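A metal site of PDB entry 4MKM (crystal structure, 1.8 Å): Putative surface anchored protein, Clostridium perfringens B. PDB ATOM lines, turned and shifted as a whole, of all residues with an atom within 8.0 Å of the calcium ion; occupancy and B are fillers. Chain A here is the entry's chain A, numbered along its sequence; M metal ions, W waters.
OD2 of Asp 267 lies within hydrogen-bond range of N of Tyr 272 (3.0 Å). The side-chain carboxylate (OD1) of Asp 267 sits close to the backbone NH (N) of Lys 270, 3.4 Å away. OD1 of Asp 275 lies within hydrogen-bond range of OG1 of Thr 268. The backbone carbonyl oxygen (O) of Ile 266 lies within hydrogen-bond range of the backbone NH (N) of Asp 275, 2.9 Å away. The side-chain hydroxyl (OG1) of Thr 276 is in hydrogen-bond range of the side-chain carboxylate (OD1) of Asp 275.
The calcium ion is bound by OD1 of Asp 269, OD1 of Asp 267, OD1 of Asp 271, water W1, O of Asn 273 and OD2 of Asp 275.
Five residues have an atom within 4 Å of the calcium ion: Asp 267, Asp 269, Asp 271, Asn 273 and Asp 275.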
ATOM      1  N   LEU A 150     -10.030   7.342   7.611  1.00  0.00           N
ATOM      2  CA  LEU A 150     -10.960   6.248   7.310  1.00  0.00           C
ATOM      3  C   LEU A 150     -12.129   6.765   6.503  1.00  0.00           C
ATOM      4  O   LEU A 150     -12.508   7.930   6.657  1.00  0.00           O
ATOM      5  CB  LEU A 150     -11.435   5.574   8.617  1.00  0.00           C
ATOM      6  CG  LEU A 150     -10.310   4.920   9.464  1.00  0.00           C
ATOM      7  CD1 LEU A 150     -10.885   4.202  10.707  1.00  0.00           C
ATOM      8  CD2 LEU A 150      -9.484   3.930   8.640  1.00  0.00           C
ATOM      9  N   ILE A 266     -15.498  -0.294   7.235  1.00  0.00           N
ATOM     10  CA  ILE A 266     -15.928   0.241   8.525  1.00  0.00           C
ATOM     11  C   ILE A 266     -15.086  -0.353   9.654  1.00  0.00           C
ATOM     12  O   ILE A 266     -14.835  -1.559   9.664  1.00  0.00           O
ATOM     13  CB  ILE A 266     -17.439  -0.039   8.797  1.00  0.00           C
ATOM     14  CG1 ILE A 266     -18.337   0.247   7.540  1.00  0.00           C
ATOM     15  CG2 ILE A 266     -17.910   0.764  10.024  1.00  0.00           C
ATOM     16  CD1 ILE A 266     -19.529  -0.532   7.499  1.00  0.00           C
ATOM     17  N   ASP A 267     -14.732   0.496  10.608  1.00  0.00           N
ATOM     18  CA  ASP A 267     -14.040   0.138  11.847  1.00  0.00           C
ATOM     19  C   ASP A 267     -15.140   0.191  12.917  1.00  0.00           C
ATOM     20  O   ASP A 267     -15.641   1.266  13.241  1.00  0.00           O
ATOM     21  CB  ASP A 267     -12.919   1.114  12.195  1.00  0.00           C
ATOM     22  CG  ASP A 267     -12.241   0.870  13.572  1.00  0.00           C
ATOM     23  OD1 ASP A 267     -12.287  -0.292  14.070  1.00  0.00           O
ATOM     24  OD2 ASP A 267     -11.799   1.863  14.197  1.00  0.00           O
ATOM     25  N   THR A 268     -15.558  -0.958  13.406  1.00  0.00           N
ATOM     26  CA  THR A 268     -16.625  -1.088  14.417  1.00  0.00           C
ATOM     27  C   THR A 268     -16.142  -1.416  15.823  1.00  0.00           C
ATOM     28  O   THR A 268     -16.990  -1.533  16.704  1.00  0.00           O
ATOM     29  CB  THR A 268     -17.603  -2.159  13.948  1.00  0.00           C
ATOM     30  OG1 THR A 268     -16.956  -3.438  14.027  1.00  0.00           O
ATOM     31  CG2 THR A 268     -18.178  -1.874  12.552  1.00  0.00           C
ATOM     32  N   ASP A 269     -14.816  -1.540  16.064  1.00  0.00           N
ATOM     33  CA  ASP A 269     -14.272  -1.869  17.389  1.00  0.00           C
ATOM     34  C   ASP A 269     -13.223  -0.872  17.878  1.00  0.00           C
ATOM     35  O   ASP A 269     -12.482  -1.184  18.805  1.00  0.00           O
ATOM     36  CB  ASP A 269     -13.727  -3.316  17.392  1.00  0.00           C
ATOM     37  CG  ASP A 269     -12.787  -3.670  16.245  1.00  0.00           C
ATOM     38  OD1 ASP A 269     -12.240  -2.743  15.608  1.00  0.00           O
ATOM     39  OD2 ASP A 269     -12.625  -4.880  15.956  1.00  0.00           O
ATOM     40  N   LYS A 270     -13.174   0.353  17.296  1.00  0.00           N
ATOM     41  CA  LYS A 270     -12.283   1.435  17.717  1.00  0.00           C
ATOM     42  C   LYS A 270     -10.740   1.140  17.772  1.00  0.00           C
ATOM     43  O   LYS A 270     -10.034   1.779  18.551  1.00  0.00           O
ATOM     44  CB  LYS A 270     -12.770   2.019  19.074  1.00  0.00           C
ATOM     45  CG  LYS A 270     -14.127   2.733  19.005  1.00  0.00           C
ATOM     46  CD  LYS A 270     -14.468   3.378  20.368  1.00  0.00           C
ATOM     47  CE  LYS A 270     -15.524   4.467  20.274  1.00  0.00           C
ATOM     48  NZ  LYS A 270     -14.944   5.786  19.931  1.00  0.00           N
ATOM     49  N   ASP A 271     -10.218   0.228  16.931  1.00  0.00           N
ATOM     50  CA  ASP A 271      -8.783  -0.097  16.845  1.00  0.00           C
ATOM     51  C   ASP A 271      -8.115   0.543  15.604  1.00  0.00           C
ATOM     52  O   ASP A 271      -6.949   0.248  15.331  1.00  0.00           O
ATOM     53  CB  ASP A 271      -8.570  -1.632  16.839  1.00  0.00           C
ATOM     54  CG  ASP A 271      -8.990  -2.363  15.579  1.00  0.00           C
ATOM     55  OD1 ASP A 271      -9.663  -1.752  14.730  1.00  0.00           O
ATOM     56  OD2 ASP A 271      -8.618  -3.543  15.420  1.00  0.00           O
ATOM     57  N   TYR A 272      -8.867   1.354  14.823  1.00  0.00           N
ATOM     58  CA  TYR A 272      -8.405   1.973  13.567  1.00  0.00           C
ATOM     59  C   TYR A 272      -8.109   1.026  12.392  1.00  0.00           C
ATOM     60  O   TYR A 272      -7.702   1.488  11.329  1.00  0.00           O
ATOM     61  CB  TYR A 272      -7.278   2.999  13.803  1.00  0.00           C
ATOM     62  CG  TYR A 272      -7.756   4.140  14.664  1.00  0.00           C
ATOM     63  CD1 TYR A 272      -8.591   5.109  14.140  1.00  0.00           C
ATOM     64  CD2 TYR A 272      -7.525   4.153  16.032  1.00  0.00           C
ATOM     65  CE1 TYR A 272      -9.106   6.121  14.939  1.00  0.00           C
ATOM     66  CE2 TYR A 272      -8.033   5.167  16.838  1.00  0.00           C
ATOM     67  CZ  TYR A 272      -8.842   6.139  16.290  1.00  0.00           C
ATOM     68  OH  TYR A 272      -9.366   7.158  17.055  1.00  0.00           O
ATOM     69  N   ASN A 273      -8.406  -0.276  12.547  1.00  0.00           N
ATOM     70  CA  ASN A 273      -8.285  -1.275  11.486  1.00  0.00           C
ATOM     71  C   ASN A 273      -9.705  -1.565  11.026  1.00  0.00           C
ATOM     72  O   ASN A 273     -10.575  -1.863  11.871  1.00  0.00           O
ATOM     73  CB  ASN A 273      -7.646  -2.563  11.983  1.00  0.00           C
ATOM     74  CG  ASN A 273      -6.281  -2.424  12.593  1.00  0.00           C
ATOM     75  OD1 ASN A 273      -6.058  -2.839  13.735  1.00  0.00           O
ATOM     76  ND2 ASN A 273      -5.326  -1.893  11.825  1.00  0.00           N
ATOM     77  N   LEU A 274      -9.932  -1.486   9.689  1.00  0.00           N
ATOM     78  CA  LEU A 274     -11.222  -1.706   9.029  1.00  0.00           C
ATOM     79  C   LEU A 274     -11.556  -3.191   9.067  1.00  0.00           C
ATOM     80  O   LEU A 274     -10.761  -4.001   8.599  1.00  0.00           O
ATOM     81  CB  LEU A 274     -11.200  -1.194   7.565  1.00  0.00           C
ATOM     82  CG  LEU A 274     -10.914   0.308   7.404  1.00  0.00           C
ATOM     83  CD1 LEU A 274     -10.740   0.674   5.957  1.00  0.00           C
ATOM     84  CD2 LEU A 274     -12.000   1.136   8.021  1.00  0.00           C
ATOM     85  N   ASP A 275     -12.737  -3.519   9.611  1.00  0.00           N
ATOM     86  CA  ASP A 275     -13.184  -4.898   9.890  1.00  0.00           C
ATOM     87  C   ASP A 275     -14.594  -5.310   9.366  1.00  0.00           C
ATOM     88  O   ASP A 275     -14.938  -6.484   9.508  1.00  0.00           O
ATOM     89  CB  ASP A 275     -13.141  -5.117  11.409  1.00  0.00           C
ATOM     90  CG  ASP A 275     -14.022  -4.155  12.207  1.00  0.00           C
ATOM     91  OD1 ASP A 275     -15.238  -4.349  12.238  1.00  0.00           O
ATOM     92  OD2 ASP A 275     -13.476  -3.194  12.774  1.00  0.00           O
ATOM     93  N   THR A 276     -15.421  -4.366   8.855  1.00  0.00           N
ATOM     94  CA  THR A 276     -16.786  -4.679   8.419  1.00  0.00           C
ATOM     95  C   THR A 276     -17.033  -4.114   6.993  1.00  0.00           C
ATOM     96  O   THR A 276     -16.643  -2.989   6.672  1.00  0.00           O
ATOM     97  CB  THR A 276     -17.791  -4.161   9.492  1.00  0.00           C
ATOM     98  OG1 THR A 276     -17.614  -4.871  10.712  1.00  0.00           O
ATOM     99  CG2 THR A 276     -19.243  -4.275   9.050  1.00  0.00           C
HETATM  100 CA    CA M   1     -11.545  -2.308  13.816  1.00  0.00          CA
HETATM  101  O   HOH W   1     -10.386  -4.128  13.323  1.00  0.00           O
